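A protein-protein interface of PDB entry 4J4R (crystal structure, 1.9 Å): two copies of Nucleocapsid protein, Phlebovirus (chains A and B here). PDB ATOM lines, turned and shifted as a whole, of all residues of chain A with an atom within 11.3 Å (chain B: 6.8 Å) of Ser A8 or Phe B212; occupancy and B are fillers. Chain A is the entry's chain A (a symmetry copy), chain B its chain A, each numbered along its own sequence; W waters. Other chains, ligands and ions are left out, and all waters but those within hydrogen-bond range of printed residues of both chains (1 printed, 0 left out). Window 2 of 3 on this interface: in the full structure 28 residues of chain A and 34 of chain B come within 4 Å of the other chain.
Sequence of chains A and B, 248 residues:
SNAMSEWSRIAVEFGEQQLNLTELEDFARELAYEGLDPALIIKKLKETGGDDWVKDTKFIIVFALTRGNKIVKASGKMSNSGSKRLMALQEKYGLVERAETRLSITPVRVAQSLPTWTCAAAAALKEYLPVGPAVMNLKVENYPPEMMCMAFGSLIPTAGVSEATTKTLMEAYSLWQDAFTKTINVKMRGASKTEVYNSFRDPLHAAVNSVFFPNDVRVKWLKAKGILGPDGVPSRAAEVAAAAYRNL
Trp A7 touches Ala B39.
Trp A7 touches Phe B212.
CG2 of Ile B42 touches CG2 of Ile A10, at 3.8 Å.
CD1 of Ile B42 touches CB of Ala A11, 3.95 Å away.
Ala A11 touches Ser B113.
Phe B212 touches Ala A11 (CE2 to CB, 3.6 Å).
CE1 of Phe B213 touches CG2 of Val A12, 3.95 Å away.
CD2 of Leu B114 touches CE2 of Phe A14 (3.4 Å).
Water W1 bridges O of Ala A11 and O of Leu B114.
Of the printed residues of chain B, Trp A7 touches Ala B39 (3.7 Å) and Phe B212 (3.5 Å).
Of chain B, only Phe B212 comes within 4 Å of Ser A8.
Of the printed residues of chain B, Phe A14 touches Leu B114 (3.4 Å).
Ser B113 touches just one residue of chain A: Ala A11 (3.6 Å).
Pro B115 touches none of the printed residues of chain A.
No residue of chain A comes within 4 Å of Ser B210.
No residue of chain A comes within 4 Å of Val B211.
Arg B218 touches none of the printed residues of chain A.
The backbone NH (N) of Ala B39 sits close to the side-chain carboxylate (OD1) of Asp B37 (3.4 Å).
The backbone NH (N) of Phe B212 is in hydrogen-bond range of the side-chain hydroxyl (OG) of Ser B210.
O of Phe B213 is in hydrogen-bond range of NE of Arg B218, at 2.7 Å.
OG of Ser A5 sits close to N of Trp A7 (3.5 Å).
OG of Ser A5 sits at hydrogen-bond distance from N of Ser A8 (3.2 Å).
Hydrophobic or aromatic side chains of chain A that line the printed part of chain B: Trp A7, Ile A10, Ala A11, Val A12 and Phe A14.
Along chain A the printed residues that touch a printed residue of chain B span positions 7 to 14.
Of the 16 printed residues of chain B, 6 touch a printed residue of chain A.
Hydrophobic or aromatic side chains of chain B within 4 Å of the printed part of chain A: Ala B39, Ile B42, Leu B114, Phe B212 and Phe B213.
Among the printed residues, 9 pairs touch across the chains.
Among the printed residues, no Asp or Glu carboxylate lies within 4 Å of a Lys or Arg side-chain nitrogen of the other chain.
The side-chain hydroxyl (OG) of Ser A8 is in hydrogen-bond range of the backbone carbonyl oxygen (O) of Phe B212 (2.4 Å).
No position is printed for both chains.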
ATOM      1  N   SER A   1      22.821  21.477  25.950  1.00  0.00           N
ATOM      2  CA  SER A   1      22.954  21.521  27.402  1.00  0.00           C
ATOM      3  C   SER A   1      23.099  22.937  27.960  1.00  0.00           C
ATOM      4  O   SER A   1      23.338  23.093  29.159  1.00  0.00           O
ATOM      5  CB  SER A   1      24.124  20.656  27.875  1.00  0.00           C
ATOM      6  OG  SER A   1      24.443  20.915  29.231  1.00  0.00           O
ATOM      7  N   ASN A   2      22.957  23.965  27.119  1.00  0.00           N
ATOM      8  CA  ASN A   2      22.928  25.338  27.634  1.00  0.00           C
ATOM      9  C   ASN A   2      21.545  25.661  28.189  1.00  0.00           C
ATOM     10  O   ASN A   2      20.561  25.034  27.794  1.00  0.00           O
ATOM     11  CB  ASN A   2      23.280  26.359  26.544  1.00  0.00           C
ATOM     12  CG  ASN A   2      24.774  26.527  26.347  1.00  0.00           C
ATOM     13  OD1 ASN A   2      25.579  26.099  27.178  1.00  0.00           O
ATOM     14  ND2 ASN A   2      25.152  27.170  25.241  1.00  0.00           N
ATOM     15  N   ALA A   3      21.466  26.644  29.087  1.00  0.00           N
ATOM     16  CA  ALA A   3      20.176  27.089  29.632  1.00  0.00           C
ATOM     17  C   ALA A   3      19.227  27.505  28.512  1.00  0.00           C
ATOM     18  O   ALA A   3      19.642  28.181  27.569  1.00  0.00           O
ATOM     19  CB  ALA A   3      20.373  28.248  30.598  1.00  0.00           C
ATOM     20  N   MET A   4      17.959  27.108  28.621  1.00  0.00           N
ATOM     21  CA  MET A   4      16.944  27.493  27.637  1.00  0.00           C
ATOM     22  C   MET A   4      15.589  27.702  28.315  1.00  0.00           C
ATOM     23  O   MET A   4      15.409  27.321  29.479  1.00  0.00           O
ATOM     24  CB  MET A   4      16.837  26.413  26.555  1.00  0.00           C
ATOM     25  CG  MET A   4      16.441  25.053  27.116  1.00  0.00           C
ATOM     26  SD  MET A   4      16.409  23.707  25.906  1.00  0.00           S
ATOM     27  CE  MET A   4      18.054  22.997  26.087  1.00  0.00           C
ATOM     28  N   SER A   5      14.633  28.292  27.598  1.00  0.00           N
ATOM     29  CA  SER A   5      13.293  28.513  28.156  1.00  0.00           C
ATOM     30  C   SER A   5      12.534  27.197  28.309  1.00  0.00           C
ATOM     31  O   SER A   5      12.929  26.168  27.739  1.00  0.00           O
ATOM     32  CB  SER A   5      12.487  29.466  27.278  1.00  0.00           C
ATOM     33  OG  SER A   5      11.982  28.808  26.123  1.00  0.00           O
ATOM     34  N   GLU A   6      11.438  27.216  29.062  1.00  0.00           N
ATOM     35  CA  GLU A   6      10.684  25.987  29.269  1.00  0.00           C
ATOM     36  C   GLU A   6       9.976  25.528  27.982  1.00  0.00           C
ATOM     37  O   GLU A   6       9.807  24.333  27.771  1.00  0.00           O
ATOM     38  CB  GLU A   6       9.721  26.090  30.466  1.00  0.00           C
ATOM     39  CG  GLU A   6      10.406  26.361  31.841  1.00  0.00           C
ATOM     40  CD  GLU A   6      10.966  25.099  32.524  1.00  0.00           C
ATOM     41  OE1 GLU A   6      10.868  24.003  31.932  1.00  0.00           O
ATOM     42  OE2 GLU A   6      11.507  25.183  33.665  1.00  0.00           O
ATOM     43  N   TRP A   7       9.595  26.457  27.106  1.00  0.00           N
ATOM     44  CA  TRP A   7       9.011  26.035  25.828  1.00  0.00           C
ATOM     45  C   TRP A   7      10.047  25.416  24.885  1.00  0.00           C
ATOM     46  O   TRP A   7       9.751  24.431  24.202  1.00  0.00           O
ATOM     47  CB  TRP A   7       8.243  27.179  25.151  1.00  0.00           C
ATOM     48  CG  TRP A   7       7.067  27.640  25.971  1.00  0.00           C
ATOM     49  CD1 TRP A   7       6.889  28.872  26.547  1.00  0.00           C
ATOM     50  CD2 TRP A   7       5.920  26.863  26.328  1.00  0.00           C
ATOM     51  NE1 TRP A   7       5.694  28.908  27.231  1.00  0.00           N
ATOM     52  CE2 TRP A   7       5.082  27.686  27.113  1.00  0.00           C
ATOM     53  CE3 TRP A   7       5.520  25.551  26.064  1.00  0.00           C
ATOM     54  CZ2 TRP A   7       3.866  27.235  27.632  1.00  0.00           C
ATOM     55  CZ3 TRP A   7       4.317  25.107  26.577  1.00  0.00           C
ATOM     56  CH2 TRP A   7       3.505  25.947  27.356  1.00  0.00           C
ATOM     57  N   SER A   8      11.252  25.990  24.843  1.00  0.00           N
ATOM     58  CA  SER A   8      12.352  25.404  24.073  1.00  0.00           C
ATOM     59  C   SER A   8      12.687  24.001  24.576  1.00  0.00           C
ATOM     60  O   SER A   8      12.904  23.063  23.785  1.00  0.00           O
ATOM     61  CB  SER A   8      13.610  26.273  24.158  1.00  0.00           C
ATOM     62  OG  SER A   8      13.478  27.450  23.392  1.00  0.00           O
ATOM     63  N   ARG A   9      12.745  23.863  25.895  1.00  0.00           N
ATOM     64  CA  ARG A   9      13.067  22.578  26.499  1.00  0.00           C
ATOM     65  C   ARG A   9      12.067  21.485  26.118  1.00  0.00           C
ATOM     66  O   ARG A   9      12.454  20.336  25.881  1.00  0.00           O
ATOM     67  CB  ARG A   9      13.159  22.701  28.026  1.00  0.00           C
ATOM     68  CG  ARG A   9      13.601  21.402  28.666  1.00  0.00           C
ATOM     69  CD  ARG A   9      14.009  21.583  30.113  1.00  0.00           C
ATOM     70  NE  ARG A   9      12.869  21.794  30.994  1.00  0.00           N
ATOM     71  CZ  ARG A   9      12.163  20.822  31.568  1.00  0.00           C
ATOM     72  NH1 ARG A   9      12.445  19.543  31.323  1.00  0.00           N
ATOM     73  NH2 ARG A   9      11.157  21.131  32.377  1.00  0.00           N
ATOM     74  N   ILE A  10      10.786  21.849  26.060  1.00  0.00           N
ATOM     75  CA  ILE A  10       9.743  20.922  25.626  1.00  0.00           C
ATOM     76  C   ILE A  10      10.011  20.454  24.191  1.00  0.00           C
ATOM     77  O   ILE A  10       9.936  19.260  23.906  1.00  0.00           O
ATOM     78  CB  ILE A  10       8.335  21.550  25.734  1.00  0.00           C
ATOM     79  CG1 ILE A  10       7.902  21.608  27.200  1.00  0.00           C
ATOM     80  CG2 ILE A  10       7.314  20.755  24.920  1.00  0.00           C
ATOM     81  CD1 ILE A  10       6.659  22.455  27.456  1.00  0.00           C
ATOM     82  N   ALA A  11      10.334  21.388  23.303  1.00  0.00           N
ATOM     83  CA  ALA A  11      10.642  21.028  21.914  1.00  0.00           C
ATOM     84  C   ALA A  11      11.880  20.125  21.862  1.00  0.00           C
ATOM     85  O   ALA A  11      11.928  19.152  21.109  1.00  0.00           O
ATOM     86  CB  ALA A  11      10.841  22.276  21.057  1.00  0.00           C
ATOM     87  N   VAL A  12      12.880  20.442  22.676  1.00  0.00           N
ATOM     88  CA  VAL A  12      14.107  19.656  22.696  1.00  0.00           C
ATOM     89  C   VAL A  12      13.859  18.232  23.197  1.00  0.00           C
ATOM     90  O   VAL A  12      14.295  17.256  22.568  1.00  0.00           O
ATOM     91  CB  VAL A  12      15.182  20.339  23.541  1.00  0.00           C
ATOM     92  CG1 VAL A  12      16.301  19.352  23.882  1.00  0.00           C
ATOM     93  CG2 VAL A  12      15.723  21.564  22.807  1.00  0.00           C
ATOM     94  N   GLU A  13      13.142  18.111  24.309  1.00  0.00           N
ATOM     95  CA  GLU A  13      12.854  16.794  24.883  1.00  0.00           C
ATOM     96  C   GLU A  13      11.897  15.968  24.020  1.00  0.00           C
ATOM     97  O   GLU A  13      12.010  14.742  23.954  1.00  0.00           O
ATOM     98  CB  GLU A  13      12.327  16.946  26.311  1.00  0.00           C
ATOM     99  CG  GLU A  13      13.437  17.347  27.282  1.00  0.00           C
ATOM    100  CD  GLU A  13      12.951  17.481  28.699  1.00  0.00           C
ATOM    101  OE1 GLU A  13      13.618  18.197  29.475  1.00  0.00           O
ATOM    102  OE2 GLU A  13      11.918  16.855  29.039  1.00  0.00           O
ATOM    103  N   PHE A  14      10.952  16.635  23.364  1.00  0.00           N
ATOM    104  CA  PHE A  14      10.078  15.955  22.413  1.00  0.00           C
ATOM    105  C   PHE A  14      10.938  15.217  21.381  1.00  0.00           C
ATOM    106  O   PHE A  14      10.663  14.061  21.025  1.00  0.00           O
ATOM    107  CB  PHE A  14       9.181  16.971  21.701  1.00  0.00           C
ATOM    108  CG  PHE A  14       7.935  16.370  21.095  1.00  0.00           C
ATOM    109  CD1 PHE A  14       6.694  16.547  21.708  1.00  0.00           C
ATOM    110  CD2 PHE A  14       8.000  15.634  19.916  1.00  0.00           C
ATOM    111  CE1 PHE A  14       5.537  15.992  21.153  1.00  0.00           C
ATOM    112  CE2 PHE A  14       6.847  15.086  19.357  1.00  0.00           C
ATOM    113  CZ  PHE A  14       5.619  15.267  19.976  1.00  0.00           C
ATOM    114  N   GLY A  15      11.985  15.882  20.905  1.00  0.00           N
ATOM    115  CA  GLY A  15      12.860  15.307  19.896  1.00  0.00           C
ATOM    116  C   GLY A  15      13.873  14.316  20.430  1.00  0.00           C
ATOM    117  O   GLY A  15      14.591  13.687  19.651  1.00  0.00           O
ATOM    118  N   GLU A  16      13.955  14.166  21.748  1.00  0.00           N
ATOM    119  CA  GLU A  16      14.854  13.154  22.306  1.00  0.00           C
ATOM    120  C   GLU A  16      14.149  11.807  22.459  1.00  0.00           C
ATOM    121  O   GLU A  16      14.790  10.807  22.786  1.00  0.00           O
ATOM    122  CB  GLU A  16      15.461  13.619  23.644  1.00  0.00           C
ATOM    123  CG  GLU A  16      16.362  14.843  23.501  1.00  0.00           C
ATOM    124  CD  GLU A  16      16.943  15.328  24.820  1.00  0.00           C
ATOM    125  OE1 GLU A  16      16.181  15.827  25.671  1.00  0.00           O
ATOM    126  OE2 GLU A  16      18.174  15.227  25.004  1.00  0.00           O
ATOM    127  N   ASP B  37       5.522  31.260  15.422  1.00  0.00           N
ATOM    128  CA  ASP B  37       5.937  31.333  16.808  1.00  0.00           C
ATOM    129  C   ASP B  37       5.805  29.924  17.411  1.00  0.00           C
ATOM    130  O   ASP B  37       4.709  29.501  17.801  1.00  0.00           O
ATOM    131  CB  ASP B  37       5.022  32.320  17.531  1.00  0.00           C
ATOM    132  CG  ASP B  37       5.454  32.586  18.946  1.00  0.00           C
ATOM    133  OD1 ASP B  37       6.236  31.778  19.507  1.00  0.00           O
ATOM    134  OD2 ASP B  37       5.005  33.610  19.516  1.00  0.00           O
ATOM    135  N   PRO B  38       6.922  29.187  17.481  1.00  0.00           N
ATOM    136  CA  PRO B  38       6.839  27.788  17.912  1.00  0.00           C
ATOM    137  C   PRO B  38       6.373  27.637  19.358  1.00  0.00           C
ATOM    138  O   PRO B  38       5.648  26.692  19.640  1.00  0.00           O
ATOM    139  CB  PRO B  38       8.281  27.278  17.769  1.00  0.00           C
ATOM    140  CG  PRO B  38       8.952  28.250  16.855  1.00  0.00           C
ATOM    141  CD  PRO B  38       8.286  29.569  17.075  1.00  0.00           C
ATOM    142  N   ALA B  39       6.773  28.542  20.253  1.00  0.00           N
ATOM    143  CA  ALA B  39       6.339  28.444  21.644  1.00  0.00           C
ATOM    144  C   ALA B  39       4.816  28.582  21.748  1.00  0.00           C
ATOM    145  O   ALA B  39       4.177  27.904  22.548  1.00  0.00           O
ATOM    146  CB  ALA B  39       7.033  29.494  22.494  1.00  0.00           C
ATOM    147  N   LEU B  40       4.250  29.467  20.934  1.00  0.00           N
ATOM    148  CA  LEU B  40       2.800  29.679  20.891  1.00  0.00           C
ATOM    149  C   LEU B  40       2.078  28.411  20.447  1.00  0.00           C
ATOM    150  O   LEU B  40       1.112  27.987  21.081  1.00  0.00           O
ATOM    151  CB  LEU B  40       2.469  30.845  19.962  1.00  0.00           C
ATOM    152  CG  LEU B  40       1.003  31.249  19.796  1.00  0.00           C
ATOM    153  CD1 LEU B  40       0.335  31.366  21.164  1.00  0.00           C
ATOM    154  CD2 LEU B  40       0.895  32.573  19.045  1.00  0.00           C
ATOM    155  N   ILE B  42       3.200  25.251  20.522  1.00  0.00           N
ATOM    156  CA  ILE B  42       3.353  24.176  21.493  1.00  0.00           C
ATOM    157  C   ILE B  42       2.456  24.394  22.722  1.00  0.00           C
ATOM    158  O   ILE B  42       1.863  23.446  23.255  1.00  0.00           O
ATOM    159  CB  ILE B  42       4.827  24.009  21.910  1.00  0.00           C
ATOM    160  CG1 ILE B  42       5.657  23.568  20.697  1.00  0.00           C
ATOM    161  CG2 ILE B  42       4.955  22.987  23.023  1.00  0.00           C
ATOM    162  CD1 ILE B  42       7.145  23.672  20.898  1.00  0.00           C
ATOM    163  N   GLN B 112       7.175  22.094  12.257  1.00  0.00           N
ATOM    164  CA  GLN B 112       8.309  23.001  12.355  1.00  0.00           C
ATOM    165  C   GLN B 112       8.606  23.394  13.796  1.00  0.00           C
ATOM    166  O   GLN B 112       9.733  23.778  14.116  1.00  0.00           O
ATOM    167  CB  GLN B 112       8.088  24.246  11.467  1.00  0.00           C
ATOM    168  CG  GLN B 112       8.225  23.970   9.958  1.00  0.00           C
ATOM    169  CD  GLN B 112       7.799  25.153   9.109  1.00  0.00           C
ATOM    170  OE1 GLN B 112       6.982  25.976   9.540  1.00  0.00           O
ATOM    171  NE2 GLN B 112       8.358  25.256   7.900  1.00  0.00           N
ATOM    172  N   SER B 113       7.613  23.284  14.676  1.00  0.00           N
ATOM    173  CA  SER B 113       7.810  23.654  16.076  1.00  0.00           C
ATOM    174  C   SER B 113       8.562  22.583  16.857  1.00  0.00           C
ATOM    175  O   SER B 113       9.083  22.830  17.946  1.00  0.00           O
ATOM    176  CB  SER B 113       6.473  23.939  16.756  1.00  0.00           C
ATOM    177  OG  SER B 113       5.829  25.020  16.112  1.00  0.00           O
ATOM    178  N   LEU B 114       8.598  21.378  16.305  1.00  0.00           N
ATOM    179  CA  LEU B 114       9.259  20.258  16.958  1.00  0.00           C
ATOM    180  C   LEU B 114      10.282  19.659  15.986  1.00  0.00           C
ATOM    181  O   LEU B 114      10.167  18.501  15.595  1.00  0.00           O
ATOM    182  CB  LEU B 114       8.222  19.205  17.356  1.00  0.00           C
ATOM    183  CG  LEU B 114       7.187  19.450  18.468  1.00  0.00           C
ATOM    184  CD1 LEU B 114       6.386  20.717  18.347  1.00  0.00           C
ATOM    185  CD2 LEU B 114       6.211  18.332  18.459  1.00  0.00           C
ATOM    186  N   PRO B 115      11.300  20.447  15.600  1.00  0.00           N
ATOM    187  CA  PRO B 115      11.999  20.063  14.364  1.00  0.00           C
ATOM    188  C   PRO B 115      12.873  18.813  14.471  1.00  0.00           C
ATOM    189  O   PRO B 115      13.005  18.101  13.470  1.00  0.00           O
ATOM    190  CB  PRO B 115      12.845  21.310  14.035  1.00  0.00           C
ATOM    191  CG  PRO B 115      13.053  21.992  15.384  1.00  0.00           C
ATOM    192  CD  PRO B 115      11.783  21.733  16.150  1.00  0.00           C
ATOM    193  N   ASN B 209      17.807  31.666  11.630  1.00  0.00           N
ATOM    194  CA  ASN B 209      18.064  32.750  12.588  1.00  0.00           C
ATOM    195  C   ASN B 209      17.243  32.710  13.876  1.00  0.00           C
ATOM    196  O   ASN B 209      17.490  33.496  14.795  1.00  0.00           O
ATOM    197  CB  ASN B 209      17.869  34.126  11.921  1.00  0.00           C
ATOM    198  CG  ASN B 209      18.941  34.441  10.898  1.00  0.00           C
ATOM    199  OD1 ASN B 209      20.075  33.979  11.009  1.00  0.00           O
ATOM    200  ND2 ASN B 209      18.588  35.248   9.894  1.00  0.00           N
ATOM    201  N   SER B 210      16.270  31.812  13.948  1.00  0.00           N
ATOM    202  CA  SER B 210      15.417  31.702  15.130  1.00  0.00           C
ATOM    203  C   SER B 210      16.215  31.372  16.396  1.00  0.00           C
ATOM    204  O   SER B 210      17.140  30.554  16.362  1.00  0.00           O
ATOM    205  CB  SER B 210      14.358  30.624  14.921  1.00  0.00           C
ATOM    206  OG  SER B 210      13.538  30.519  16.070  1.00  0.00           O
ATOM    207  N   VAL B 211      15.853  31.992  17.513  1.00  0.00           N
ATOM    208  CA  VAL B 211      16.523  31.677  18.774  1.00  0.00           C
ATOM    209  C   VAL B 211      15.755  30.639  19.596  1.00  0.00           C
ATOM    210  O   VAL B 211      16.217  30.218  20.652  1.00  0.00           O
ATOM    211  CB  VAL B 211      16.795  32.945  19.626  1.00  0.00           C
ATOM    212  CG1 VAL B 211      17.618  33.943  18.840  1.00  0.00           C
ATOM    213  CG2 VAL B 211      15.479  33.583  20.077  1.00  0.00           C
ATOM    214  N   PHE B 212      14.584  30.229  19.115  1.00  0.00           N
ATOM    215  CA  PHE B 212      13.754  29.301  19.879  1.00  0.00           C
ATOM    216  C   PHE B 212      14.459  27.950  20.084  1.00  0.00           C
ATOM    217  O   PHE B 212      14.569  27.451  21.210  1.00  0.00           O
ATOM    218  CB  PHE B 212      12.381  29.108  19.217  1.00  0.00           C
ATOM    219  CG  PHE B 212      11.567  28.001  19.841  1.00  0.00           C
ATOM    220  CD1 PHE B 212      10.858  28.218  21.016  1.00  0.00           C
ATOM    221  CD2 PHE B 212      11.531  26.739  19.261  1.00  0.00           C
ATOM    222  CE1 PHE B 212      10.114  27.188  21.603  1.00  0.00           C
ATOM    223  CE2 PHE B 212      10.791  25.703  19.842  1.00  0.00           C
ATOM    224  CZ  PHE B 212      10.082  25.933  21.008  1.00  0.00           C
ATOM    225  N   PHE B 213      14.952  27.370  18.998  1.00  0.00           N
ATOM    226  CA  PHE B 213      15.605  26.069  19.071  1.00  0.00           C
ATOM    227  C   PHE B 213      17.127  26.212  19.145  1.00  0.00           C
ATOM    228  O   PHE B 213      17.780  26.572  18.159  1.00  0.00           O
ATOM    229  CB  PHE B 213      15.197  25.174  17.895  1.00  0.00           C
ATOM    230  CG  PHE B 213      15.335  23.714  18.194  1.00  0.00           C
ATOM    231  CD1 PHE B 213      14.289  23.013  18.761  1.00  0.00           C
ATOM    232  CD2 PHE B 213      16.533  23.053  17.952  1.00  0.00           C
ATOM    233  CE1 PHE B 213      14.424  21.654  19.075  1.00  0.00           C
ATOM    234  CE2 PHE B 213      16.679  21.707  18.257  1.00  0.00           C
ATOM    235  CZ  PHE B 213      15.623  21.004  18.820  1.00  0.00           C
ATOM    236  N   PRO B 214      17.697  25.894  20.316  1.00  0.00           N
ATOM    237  CA  PRO B 214      19.078  26.263  20.670  1.00  0.00           C
ATOM    238  C   PRO B 214      20.127  25.704  19.696  1.00  0.00           C
ATOM    239  O   PRO B 214      20.044  24.529  19.311  1.00  0.00           O
ATOM    240  CB  PRO B 214      19.262  25.645  22.062  1.00  0.00           C
ATOM    241  CG  PRO B 214      17.866  25.435  22.592  1.00  0.00           C
ATOM    242  CD  PRO B 214      17.040  25.107  21.379  1.00  0.00           C
ATOM    243  N   ARG B 218      21.176  21.783  18.043  1.00  0.00           N
ATOM    244  CA  ARG B 218      21.244  21.556  16.599  1.00  0.00           C
ATOM    245  C   ARG B 218      22.551  20.880  16.197  1.00  0.00           C
ATOM    246  O   ARG B 218      22.546  19.876  15.485  1.00  0.00           O
ATOM    247  CB  ARG B 218      21.139  22.872  15.823  1.00  0.00           C
ATOM    248  CG  ARG B 218      19.876  23.670  16.078  1.00  0.00           C
ATOM    249  CD  ARG B 218      19.856  24.920  15.224  1.00  0.00           C
ATOM    250  NE  ARG B 218      19.074  25.985  15.846  1.00  0.00           N
ATOM    251  CZ  ARG B 218      18.826  27.161  15.272  1.00  0.00           C
ATOM    252  NH1 ARG B 218      19.283  27.418  14.052  1.00  0.00           N
ATOM    253  NH2 ARG B 218      18.120  28.083  15.920  1.00  0.00           N
HETATM  254  O   HOH W   1      11.746  18.563  18.365  1.00  0.00           O
